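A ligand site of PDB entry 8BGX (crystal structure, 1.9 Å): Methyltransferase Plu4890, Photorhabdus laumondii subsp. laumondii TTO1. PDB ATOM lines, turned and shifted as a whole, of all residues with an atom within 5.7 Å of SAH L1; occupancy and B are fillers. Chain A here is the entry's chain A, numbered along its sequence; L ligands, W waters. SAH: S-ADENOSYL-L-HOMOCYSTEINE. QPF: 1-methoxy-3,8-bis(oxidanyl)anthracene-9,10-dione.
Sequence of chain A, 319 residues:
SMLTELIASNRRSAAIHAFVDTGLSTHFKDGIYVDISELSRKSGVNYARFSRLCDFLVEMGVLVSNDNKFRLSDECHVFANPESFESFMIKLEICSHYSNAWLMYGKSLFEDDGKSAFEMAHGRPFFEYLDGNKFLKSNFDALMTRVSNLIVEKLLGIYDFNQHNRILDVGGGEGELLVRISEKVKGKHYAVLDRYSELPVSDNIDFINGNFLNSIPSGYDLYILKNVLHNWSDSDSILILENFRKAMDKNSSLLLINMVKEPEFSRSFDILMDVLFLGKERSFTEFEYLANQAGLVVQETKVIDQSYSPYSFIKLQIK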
ATOM      1  N   PHE A 127     -28.096  13.123  15.563  1.00  0.00           N
ATOM      2  CA  PHE A 127     -29.350  13.529  16.254  1.00  0.00           C
ATOM      3  C   PHE A 127     -30.554  12.870  15.577  1.00  0.00           C
ATOM      4  O   PHE A 127     -31.449  12.411  16.312  1.00  0.00           O
ATOM      5  CB  PHE A 127     -29.439  15.058  16.371  1.00  0.00           C
ATOM      6  CG  PHE A 127     -28.492  15.629  17.402  1.00  0.00           C
ATOM      7  CD1 PHE A 127     -28.571  15.219  18.726  1.00  0.00           C
ATOM      8  CD2 PHE A 127     -27.510  16.536  17.043  1.00  0.00           C
ATOM      9  CE1 PHE A 127     -27.694  15.725  19.680  1.00  0.00           C
ATOM     10  CE2 PHE A 127     -26.640  17.049  18.000  1.00  0.00           C
ATOM     11  CZ  PHE A 127     -26.731  16.636  19.306  1.00  0.00           C
ATOM     12  N   LYS A 137     -30.347   8.194  22.953  1.00  0.00           N
ATOM     13  CA  LYS A 137     -31.059   9.474  23.204  1.00  0.00           C
ATOM     14  C   LYS A 137     -31.169   9.715  24.709  1.00  0.00           C
ATOM     15  O   LYS A 137     -30.737  10.804  25.148  1.00  0.00           O
ATOM     16  CB  LYS A 137     -32.446   9.509  22.551  1.00  0.00           C
ATOM     17  CG  LYS A 137     -33.222  10.798  22.806  1.00  0.00           C
ATOM     18  CD  LYS A 137     -34.189  11.186  21.718  1.00  0.00           C
ATOM     19  CE  LYS A 137     -34.804  12.554  21.931  1.00  0.00           C
ATOM     20  NZ  LYS A 137     -33.792  13.643  21.789  1.00  0.00           N
ATOM     21  N   PHE A 140     -27.533  10.236  26.243  1.00  0.00           N
ATOM     22  CA  PHE A 140     -26.928  11.495  25.735  1.00  0.00           C
ATOM     23  C   PHE A 140     -27.618  12.695  26.414  1.00  0.00           C
ATOM     24  O   PHE A 140     -26.931  13.578  26.940  1.00  0.00           O
ATOM     25  CB  PHE A 140     -27.006  11.611  24.220  1.00  0.00           C
ATOM     26  CG  PHE A 140     -26.470  12.936  23.744  1.00  0.00           C
ATOM     27  CD1 PHE A 140     -25.108  13.150  23.651  1.00  0.00           C
ATOM     28  CD2 PHE A 140     -27.327  13.996  23.494  1.00  0.00           C
ATOM     29  CE1 PHE A 140     -24.609  14.385  23.251  1.00  0.00           C
ATOM     30  CE2 PHE A 140     -26.821  15.235  23.100  1.00  0.00           C
ATOM     31  CZ  PHE A 140     -25.467  15.421  22.984  1.00  0.00           C
ATOM     32  N   ASP A 141     -28.955  12.709  26.403  1.00  0.00           N
ATOM     33  CA  ASP A 141     -29.767  13.798  27.021  1.00  0.00           C
ATOM     34  C   ASP A 141     -29.453  13.867  28.527  1.00  0.00           C
ATOM     35  O   ASP A 141     -29.308  14.991  29.037  1.00  0.00           O
ATOM     36  CB  ASP A 141     -31.251  13.612  26.739  1.00  0.00           C
ATOM     37  CG  ASP A 141     -31.654  13.984  25.320  1.00  0.00           C
ATOM     38  OD1 ASP A 141     -30.791  14.528  24.589  1.00  0.00           O
ATOM     39  OD2 ASP A 141     -32.805  13.716  24.944  1.00  0.00           O
ATOM     40  N   MET A 144     -26.018  15.495  29.043  1.00  0.00           N
ATOM     41  CA  MET A 144     -26.157  16.965  28.839  1.00  0.00           C
ATOM     42  C   MET A 144     -26.815  17.595  30.068  1.00  0.00           C
ATOM     43  O   MET A 144     -26.361  18.681  30.498  1.00  0.00           O
ATOM     44  CB  MET A 144     -26.995  17.278  27.588  1.00  0.00           C
ATOM     45  CG  MET A 144     -26.370  16.799  26.286  1.00  0.00           C
ATOM     46  SD  MET A 144     -24.671  17.364  26.027  1.00  0.00           S
ATOM     47  CE  MET A 144     -23.767  15.906  26.539  1.00  0.00           C
ATOM     48  N   THR A 145     -27.835  16.943  30.631  1.00  0.00           N
ATOM     49  CA  THR A 145     -28.536  17.375  31.867  1.00  0.00           C
ATOM     50  C   THR A 145     -27.542  17.476  33.031  1.00  0.00           C
ATOM     51  O   THR A 145     -27.595  18.485  33.762  1.00  0.00           O
ATOM     52  CB  THR A 145     -29.729  16.445  32.170  1.00  0.00           C
ATOM     53  OG1 THR A 145     -30.749  16.755  31.227  1.00  0.00           O
ATOM     54  CG2 THR A 145     -30.275  16.607  33.575  1.00  0.00           C
ATOM     55  N   VAL A 147     -24.169  17.859  32.994  1.00  0.00           N
ATOM     56  CA  VAL A 147     -23.115  18.910  32.772  1.00  0.00           C
ATOM     57  C   VAL A 147     -23.759  20.298  32.853  1.00  0.00           C
ATOM     58  O   VAL A 147     -23.061  21.247  33.266  1.00  0.00           O
ATOM     59  CB  VAL A 147     -22.345  18.693  31.457  1.00  0.00           C
ATOM     60  CG1 VAL A 147     -21.523  17.412  31.498  1.00  0.00           C
ATOM     61  CG2 VAL A 147     -23.241  18.710  30.226  1.00  0.00           C
ATOM     62  N   SER A 148     -25.037  20.425  32.484  1.00  0.00           N
ATOM     63  CA  SER A 148     -25.830  21.672  32.666  1.00  0.00           C
ATOM     64  C   SER A 148     -25.967  21.963  34.164  1.00  0.00           C
ATOM     65  O   SER A 148     -25.737  23.121  34.566  1.00  0.00           O
ATOM     66  CB  SER A 148     -27.173  21.579  31.993  1.00  0.00           C
ATOM     67  OG  SER A 148     -27.044  21.688  30.585  1.00  0.00           O
ATOM     68  N   ASP A 169     -33.849  29.231  26.022  1.00  0.00           N
ATOM     69  CA  ASP A 169     -32.676  28.323  25.879  1.00  0.00           C
ATOM     70  C   ASP A 169     -32.871  27.510  24.599  1.00  0.00           C
ATOM     71  O   ASP A 169     -33.824  26.710  24.551  1.00  0.00           O
ATOM     72  CB  ASP A 169     -32.498  27.434  27.115  1.00  0.00           C
ATOM     73  CG  ASP A 169     -31.169  26.704  27.153  1.00  0.00           C
ATOM     74  OD1 ASP A 169     -30.337  26.960  26.265  1.00  0.00           O
ATOM     75  OD2 ASP A 169     -30.972  25.891  28.083  1.00  0.00           O
ATOM     76  N   VAL A 170     -32.008  27.719  23.596  1.00  0.00           N
ATOM     77  CA  VAL A 170     -32.125  27.130  22.235  1.00  0.00           C
ATOM     78  C   VAL A 170     -31.240  25.880  22.162  1.00  0.00           C
ATOM     79  O   VAL A 170     -30.044  25.986  22.468  1.00  0.00           O
ATOM     80  CB  VAL A 170     -31.750  28.164  21.151  1.00  0.00           C
ATOM     81  CG1 VAL A 170     -31.666  27.538  19.761  1.00  0.00           C
ATOM     82  CG2 VAL A 170     -32.728  29.341  21.149  1.00  0.00           C
ATOM     83  N   GLY A 171     -31.831  24.753  21.745  1.00  0.00           N
ATOM     84  CA  GLY A 171     -31.198  23.420  21.840  1.00  0.00           C
ATOM     85  C   GLY A 171     -30.936  23.054  23.292  1.00  0.00           C
ATOM     86  O   GLY A 171     -29.848  22.511  23.587  1.00  0.00           O
ATOM     87  N   GLY A 172     -31.917  23.330  24.169  1.00  0.00           N
ATOM     88  CA  GLY A 172     -31.790  23.209  25.642  1.00  0.00           C
ATOM     89  C   GLY A 172     -32.033  21.803  26.154  1.00  0.00           C
ATOM     90  O   GLY A 172     -31.933  21.606  27.387  1.00  0.00           O
ATOM     91  N   GLY A 173     -32.355  20.848  25.271  1.00  0.00           N
ATOM     92  CA  GLY A 173     -32.525  19.421  25.608  1.00  0.00           C
ATOM     93  C   GLY A 173     -33.685  19.195  26.552  1.00  0.00           C
ATOM     94  O   GLY A 173     -34.797  19.625  26.219  1.00  0.00           O
ATOM     95  N   LEU A 193     -36.300  25.449  23.526  1.00  0.00           N
ATOM     96  CA  LEU A 193     -36.497  24.977  22.130  1.00  0.00           C
ATOM     97  C   LEU A 193     -35.518  23.832  21.853  1.00  0.00           C
ATOM     98  O   LEU A 193     -34.303  23.989  22.125  1.00  0.00           O
ATOM     99  CB  LEU A 193     -36.279  26.133  21.149  1.00  0.00           C
ATOM    100  CG  LEU A 193     -36.590  25.818  19.690  1.00  0.00           C
ATOM    101  CD1 LEU A 193     -37.002  27.079  18.936  1.00  0.00           C
ATOM    102  CD2 LEU A 193     -35.420  25.150  18.988  1.00  0.00           C
ATOM    103  N   ASP A 194     -36.027  22.721  21.329  1.00  0.00           N
ATOM    104  CA  ASP A 194     -35.225  21.564  20.861  1.00  0.00           C
ATOM    105  C   ASP A 194     -36.092  20.753  19.900  1.00  0.00           C
ATOM    106  O   ASP A 194     -37.197  21.235  19.570  1.00  0.00           O
ATOM    107  CB  ASP A 194     -34.722  20.749  22.066  1.00  0.00           C
ATOM    108  CG  ASP A 194     -33.421  19.990  21.823  1.00  0.00           C
ATOM    109  OD1 ASP A 194     -33.432  19.051  21.001  1.00  0.00           O
ATOM    110  OD2 ASP A 194     -32.409  20.356  22.452  1.00  0.00           O
ATOM    111  N   ARG A 195     -35.630  19.575  19.474  1.00  0.00           N
ATOM    112  CA  ARG A 195     -36.398  18.637  18.609  1.00  0.00           C
ATOM    113  C   ARG A 195     -37.112  17.619  19.508  1.00  0.00           C
ATOM    114  O   ARG A 195     -36.438  16.721  20.035  1.00  0.00           O
ATOM    115  CB  ARG A 195     -35.451  17.979  17.607  1.00  0.00           C
ATOM    116  CG  ARG A 195     -34.779  18.963  16.660  1.00  0.00           C
ATOM    117  CD  ARG A 195     -33.795  18.315  15.713  1.00  0.00           C
ATOM    118  NE  ARG A 195     -34.448  17.357  14.823  1.00  0.00           N
ATOM    119  CZ  ARG A 195     -34.487  16.046  15.012  1.00  0.00           C
ATOM    120  NH1 ARG A 195     -33.905  15.493  16.062  1.00  0.00           N
ATOM    121  NH2 ARG A 195     -35.124  15.277  14.139  1.00  0.00           N
ATOM    122  N   GLY A 210     -38.940  22.860  17.825  1.00  0.00           N
ATOM    123  CA  GLY A 210     -38.429  23.792  16.800  1.00  0.00           C
ATOM    124  C   GLY A 210     -37.239  23.227  16.053  1.00  0.00           C
ATOM    125  O   GLY A 210     -36.921  22.044  16.233  1.00  0.00           O
ATOM    126  N   ASN A 211     -36.598  24.077  15.253  1.00  0.00           N
ATOM    127  CA  ASN A 211     -35.424  23.733  14.424  1.00  0.00           C
ATOM    128  C   ASN A 211     -34.595  25.010  14.225  1.00  0.00           C
ATOM    129  O   ASN A 211     -34.988  25.829  13.366  1.00  0.00           O
ATOM    130  CB  ASN A 211     -35.849  23.096  13.105  1.00  0.00           C
ATOM    131  CG  ASN A 211     -34.676  22.660  12.245  1.00  0.00           C
ATOM    132  OD1 ASN A 211     -33.528  22.953  12.563  1.00  0.00           O
ATOM    133  ND2 ASN A 211     -34.962  21.963  11.156  1.00  0.00           N
ATOM    134  N   PHE A 212     -33.505  25.169  14.974  1.00  0.00           N
ATOM    135  CA  PHE A 212     -32.695  26.425  14.995  1.00  0.00           C
ATOM    136  C   PHE A 212     -31.973  26.623  13.658  1.00  0.00           C
ATOM    137  O   PHE A 212     -31.426  27.722  13.450  1.00  0.00           O
ATOM    138  CB  PHE A 212     -31.743  26.466  16.193  1.00  0.00           C
ATOM    139  CG  PHE A 212     -30.841  25.274  16.408  1.00  0.00           C
ATOM    140  CD1 PHE A 212     -30.754  24.687  17.667  1.00  0.00           C
ATOM    141  CD2 PHE A 212     -30.072  24.762  15.382  1.00  0.00           C
ATOM    142  CE1 PHE A 212     -29.910  23.602  17.882  1.00  0.00           C
ATOM    143  CE2 PHE A 212     -29.237  23.666  15.600  1.00  0.00           C
ATOM    144  CZ  PHE A 212     -29.153  23.098  16.847  1.00  0.00           C
ATOM    145  N   LEU A 213     -31.962  25.618  12.769  1.00  0.00           N
ATOM    146  CA  LEU A 213     -31.456  25.758  11.375  1.00  0.00           C
ATOM    147  C   LEU A 213     -32.452  26.557  10.532  1.00  0.00           C
ATOM    148  O   LEU A 213     -32.002  27.204   9.561  1.00  0.00           O
ATOM    149  CB  LEU A 213     -31.222  24.384  10.748  1.00  0.00           C
ATOM    150  CG  LEU A 213     -30.153  23.517  11.419  1.00  0.00           C
ATOM    151  CD1 LEU A 213     -30.053  22.156  10.732  1.00  0.00           C
ATOM    152  CD2 LEU A 213     -28.798  24.206  11.421  1.00  0.00           C
ATOM    153  N   LEU A 225     -27.501  29.734  23.987  1.00  0.00           N
ATOM    154  CA  LEU A 225     -27.048  28.636  23.098  1.00  0.00           C
ATOM    155  C   LEU A 225     -25.822  27.988  23.741  1.00  0.00           C
ATOM    156  O   LEU A 225     -24.706  28.506  23.533  1.00  0.00           O
ATOM    157  CB  LEU A 225     -26.742  29.227  21.722  1.00  0.00           C
ATOM    158  CG  LEU A 225     -26.542  28.199  20.595  1.00  0.00           C
ATOM    159  CD1 LEU A 225     -27.872  27.638  20.137  1.00  0.00           C
ATOM    160  CD2 LEU A 225     -25.779  28.823  19.430  1.00  0.00           C
ATOM    161  N   LYS A 226     -26.036  26.931  24.530  1.00  0.00           N
ATOM    162  CA  LYS A 226     -24.964  26.224  25.282  1.00  0.00           C
ATOM    163  C   LYS A 226     -24.625  24.890  24.609  1.00  0.00           C
ATOM    164  O   LYS A 226     -25.551  24.080  24.420  1.00  0.00           O
ATOM    165  CB  LYS A 226     -25.363  25.992  26.748  1.00  0.00           C
ATOM    166  CG  LYS A 226     -24.245  25.415  27.608  1.00  0.00           C
ATOM    167  CD  LYS A 226     -24.527  25.382  29.097  1.00  0.00           C
ATOM    168  CE  LYS A 226     -25.510  24.310  29.511  1.00  0.00           C
ATOM    169  NZ  LYS A 226     -24.902  22.961  29.462  1.00  0.00           N
ATOM    170  N   ASN A 227     -23.351  24.680  24.271  1.00  0.00           N
ATOM    171  CA  ASN A 227     -22.806  23.394  23.772  1.00  0.00           C
ATOM    172  C   ASN A 227     -23.610  22.903  22.569  1.00  0.00           C
ATOM    173  O   ASN A 227     -23.941  21.696  22.523  1.00  0.00           O
ATOM    174  CB  ASN A 227     -22.756  22.350  24.901  1.00  0.00           C
ATOM    175  CG  ASN A 227     -21.687  22.643  25.921  1.00  0.00           C
ATOM    176  OD1 ASN A 227     -20.773  23.428  25.671  1.00  0.00           O
ATOM    177  ND2 ASN A 227     -21.795  22.020  27.094  1.00  0.00           N
ATOM    178  N   VAL A 228     -23.901  23.793  21.623  1.00  0.00           N
ATOM    179  CA  VAL A 228     -24.599  23.476  20.347  1.00  0.00           C
ATOM    180  C   VAL A 228     -23.581  23.553  19.195  1.00  0.00           C
ATOM    181  O   VAL A 228     -23.461  22.553  18.461  1.00  0.00           O
ATOM    182  CB  VAL A 228     -25.798  24.411  20.099  1.00  0.00           C
ATOM    183  CG1 VAL A 228     -26.359  24.279  18.700  1.00  0.00           C
ATOM    184  CG2 VAL A 228     -26.890  24.197  21.131  1.00  0.00           C
ATOM    185  N   ASN A 231     -21.313  20.925  17.505  1.00  0.00           N
ATOM    186  CA  ASN A 231     -22.006  19.833  16.773  1.00  0.00           C
ATOM    187  C   ASN A 231     -22.191  20.190  15.282  1.00  0.00           C
ATOM    188  O   ASN A 231     -22.798  19.378  14.562  1.00  0.00           O
ATOM    189  CB  ASN A 231     -23.397  19.543  17.361  1.00  0.00           C
ATOM    190  CG  ASN A 231     -23.362  19.166  18.825  1.00  0.00           C
ATOM    191  OD1 ASN A 231     -22.402  18.559  19.295  1.00  0.00           O
ATOM    192  ND2 ASN A 231     -24.417  19.486  19.552  1.00  0.00           N
ATOM    193  N   TRP A 232     -21.694  21.356  14.832  1.00  0.00           N
ATOM    194  CA  TRP A 232     -22.055  21.923  13.504  1.00  0.00           C
ATOM    195  C   TRP A 232     -20.813  22.435  12.766  1.00  0.00           C
ATOM    196  O   TRP A 232     -19.848  22.858  13.426  1.00  0.00           O
ATOM    197  CB  TRP A 232     -23.105  23.029  13.684  1.00  0.00           C
ATOM    198  CG  TRP A 232     -24.364  22.517  14.292  1.00  0.00           C
ATOM    199  CD1 TRP A 232     -24.734  22.601  15.605  1.00  0.00           C
ATOM    200  CD2 TRP A 232     -25.390  21.759  13.636  1.00  0.00           C
ATOM    201  NE1 TRP A 232     -25.929  21.977  15.805  1.00  0.00           N
ATOM    202  CE2 TRP A 232     -26.359  21.436  14.618  1.00  0.00           C
ATOM    203  CE3 TRP A 232     -25.595  21.314  12.322  1.00  0.00           C
ATOM    204  CZ2 TRP A 232     -27.509  20.723  14.319  1.00  0.00           C
ATOM    205  CZ3 TRP A 232     -26.733  20.594  12.033  1.00  0.00           C
ATOM    206  CH2 TRP A 232     -27.684  20.304  13.018  1.00  0.00           C
HETATM  207  N   SAH L   1     -27.888  23.017  25.386  1.00  0.00           N
HETATM  208  CA  SAH L   1     -27.914  21.688  26.071  1.00  0.00           C
HETATM  209  CB  SAH L   1     -27.836  20.532  25.073  1.00  0.00           C
HETATM  210  CG  SAH L   1     -26.643  20.591  24.141  1.00  0.00           C
HETATM  211  SD  SAH L   1     -26.517  19.152  23.048  1.00  0.00           S
HETATM  212  C   SAH L   1     -26.747  21.603  27.051  1.00  0.00           C
HETATM  213  O   SAH L   1     -26.738  20.752  27.945  1.00  0.00           O
HETATM  214  OXT SAH L   1     -25.779  22.375  26.969  1.00  0.00           O
HETATM  215  C5' SAH L   1     -27.214  19.771  21.499  1.00  0.00           C
HETATM  216  C4' SAH L   1     -28.723  19.870  21.509  1.00  0.00           C
HETATM  217  O4' SAH L   1     -29.168  20.400  20.235  1.00  0.00           O
HETATM  218  C3' SAH L   1     -29.472  18.541  21.702  1.00  0.00           C
HETATM  219  O3' SAH L   1     -30.398  18.676  22.767  1.00  0.00           O
HETATM  220  C2' SAH L   1     -30.132  18.304  20.342  1.00  0.00           C
HETATM  221  O2' SAH L   1     -31.357  17.601  20.425  1.00  0.00           O
HETATM  222  C1' SAH L   1     -30.346  19.734  19.875  1.00  0.00           C
HETATM  223  N9  SAH L   1     -30.565  19.907  18.443  1.00  0.00           N
HETATM  224  C8  SAH L   1     -29.923  19.266  17.418  1.00  0.00           C
HETATM  225  N7  SAH L   1     -30.320  19.653  16.227  1.00  0.00           N
HETATM  226  C5  SAH L   1     -31.269  20.626  16.486  1.00  0.00           C
HETATM  227  C6  SAH L   1     -32.064  21.422  15.639  1.00  0.00           C
HETATM  228  N6  SAH L   1     -32.004  21.374  14.314  1.00  0.00           N
HETATM  229  N1  SAH L   1     -32.906  22.301  16.221  1.00  0.00           N
HETATM  230  C2  SAH L   1     -32.968  22.343  17.554  1.00  0.00           C
HETATM  231  N3  SAH L   1     -32.275  21.647  18.449  1.00  0.00           N
HETATM  232  C4  SAH L   1     -31.434  20.792  17.846  1.00  0.00           C
HETATM  233  OAE QPF L   2     -20.523  18.896  26.809  1.00  0.00           O
HETATM  234  CAD QPF L   2     -20.366  17.753  26.385  1.00  0.00           C
HETATM  235  CAC QPF L   2     -19.633  16.834  27.139  1.00  0.00           C
HETATM  236  CAB QPF L   2     -19.107  17.221  28.374  1.00  0.00           C
HETATM  237  CAA QPF L   2     -18.374  16.325  29.146  1.00  0.00           C
HETATM  238  CAT QPF L   2     -18.174  15.032  28.684  1.00  0.00           C
HETATM  239  CAR QPF L   2     -18.694  14.643  27.461  1.00  0.00           C
HETATM  240  OAS QPF L   2     -18.517  13.383  26.980  1.00  0.00           O
HETATM  241  CAQ QPF L   2     -19.439  15.542  26.664  1.00  0.00           C
HETATM  242  CAO QPF L   2     -19.964  15.154  25.428  1.00  0.00           C
HETATM  243  OAP QPF L   2     -19.788  14.008  25.019  1.00  0.00           O
HETATM  244  CAN QPF L   2     -20.688  16.072  24.663  1.00  0.00           C
HETATM  245  CAF QPF L   2     -20.889  17.371  25.141  1.00  0.00           C
HETATM  246  CAG QPF L   2     -21.622  18.290  24.387  1.00  0.00           C
HETATM  247  CAH QPF L   2     -22.159  17.922  23.150  1.00  0.00           C
HETATM  248  OAI QPF L   2     -22.869  18.814  22.407  1.00  0.00           O
HETATM  249  CAJ QPF L   2     -21.965  16.629  22.675  1.00  0.00           C
HETATM  250  CAK QPF L   2     -21.232  15.700  23.421  1.00  0.00           C
HETATM  251  OAL QPF L   2     -20.993  14.399  23.026  1.00  0.00           O
HETATM  252  CAM QPF L   2     -21.556  13.870  21.817  1.00  0.00           C
HETATM  253  O   HOH W   1     -29.101  19.833  28.529  1.00  0.00           O
HETATM  254  O   HOH W   2     -30.034  17.760  14.079  1.00  0.00           O
HETATM  255  O   HOH W   3     -32.242  16.199  18.316  1.00  0.00           O
HETATM  256  O   HOH W   4     -28.598  25.875  24.762  1.00  0.00           O
HETATM  257  O   HOH W   5     -26.946  20.664  18.096  1.00  0.00           O
HETATM  258  O   HOH W   6     -28.775  24.274  27.856  1.00  0.00           O
HETATM  259  O   HOH W   7     -29.795  17.163  25.178  1.00  0.00           O
HETATM  260  O   HOH W   8     -31.394  19.245  12.400  1.00  0.00           O
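Water W1 lies within hydrogen-bond range of O of SAH L1 and OG of Ser 148. Water W3 lies within hydrogen-bond range of an oxygen (O2') of SAH L1 (2.7 Å) and the guanidinium group (NH1) of Arg 195 (2.9 Å). Water W7 lies within hydrogen-bond range of OD1 of Asp 141 (2.9 Å) and O3' of SAH L1 (2.9 Å). Water W6 lies within hydrogen-bond range of OD2 of Asp 169 and N of SAH L1. Water W4 lies within hydrogen-bond range of the side-chain carboxylate (OD1) of Asp 169, the backbone carbonyl oxygen (O) of Val 170, the backbone NH (N) of Lys 226 and a nitrogen (N) of SAH L1. Water W5 lies within hydrogen-bond range of the indole nitrogen of Trp 232 (2.8 Å), an oxygen (O4') of SAH L1 (3.1 Å) and the side-chain amide nitrogen of Asn 231 (3.1 Å).
The side-chain hydroxyl (OG) of Ser 148 is in hydrogen-bond range of the backbone carbonyl oxygen (O) of Met 144, 3.1 Å away. The side-chain amino group (NZ) of Lys 226 is in hydrogen-bond range of the side-chain hydroxyl (OG) of Ser 148 (2.7 Å). The backbone carbonyl oxygen of Asp 169 sits at hydrogen-bond distance from the backbone NH of Leu 193, at 3.0 Å. OD2 of Asp 194 sits at hydrogen-bond distance from N of Gly 172. The backbone NH (N) of Gly 173 lies within hydrogen-bond range of the side-chain carboxylate (OD2) of Asp 194, at 2.9 Å. O of Leu 193 is in hydrogen-bond range of N of Gly 171, 2.6 Å away. The backbone NH (N) of Gly 172 is in hydrogen-bond range of the backbone carbonyl oxygen (O) of Leu 193 (3.2 Å). O of Asp 194 sits at hydrogen-bond distance from N of Gly 210, 3.0 Å away.
SD of SAH L1 lies close to OAI of QPF L2.
O of Met 144 sits close to O of SAH L1 (3.3 Å). O of Asn 227 sits close to SD of SAH L1, at 3.7 Å. Phe 127 touches SAH L1 (CE1 to C2', 3.6 Å). Phe 140 touches SAH L1. Gly 172 touches SAH L1 (CA to N, 3.9 Å). CA of Gly 173 touches O3' of SAH L1 (3.6 Å). CD2 of Leu 193 touches C2 of SAH L1, at 3.99 Å. CD of Arg 195 touches C5 of SAH L1, at 3.5 Å. Asn 231 touches SAH L1 (ND2 to C5', 3.4 Å). Trp 232 touches SAH L1. Hydrophobic or aromatic side chains that line SAH L1: Phe 127, Phe 140, Met 144, Leu 193, Phe 212 and Trp 232. Of the 26 residues printed, 16 come within 4 Å of SAH L1. The nearest printed residue that does not touch SAH L1 is Gly 210 (4.02 Å).
An oxygen (OXT) of SAH L1 lies within salt-bridge range of the side-chain amino group (NZ) of Lys 226. The side-chain amide nitrogen (ND2) of Asn 227 is in hydrogen-bond range of an oxygen (OAE) of QPF L2, at 3.4 Å. An oxygen (O2') of SAH L1 lies within hydrogen-bond range of the side-chain carboxylate of Asp 194 (2.6 Å). The side-chain amide oxygen (OD1) of Asn 231 sits at hydrogen-bond distance from an oxygen (OAI) of QPF L2, 3.2 Å away. The backbone carbonyl oxygen of Gly 171 sits at hydrogen-bond distance from a nitrogen (N) of SAH L1 (2.7 Å). OAI of QPF L2 is in hydrogen-bond range of O of Asn 227 (3.1 Å). OG of Ser 148 is in hydrogen-bond range of O of SAH L1, at 2.8 Å. The backbone NH (N) of Phe 212 lies within hydrogen-bond range of a nitrogen (N1) of SAH L1, 3.2 Å away. The side-chain amide oxygen of Asn 211 is in hydrogen-bond range of a nitrogen (N6) of SAH L1 (2.8 Å). O of Lys 226 is in hydrogen-bond range of N of SAH L1 (2.7 Å).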
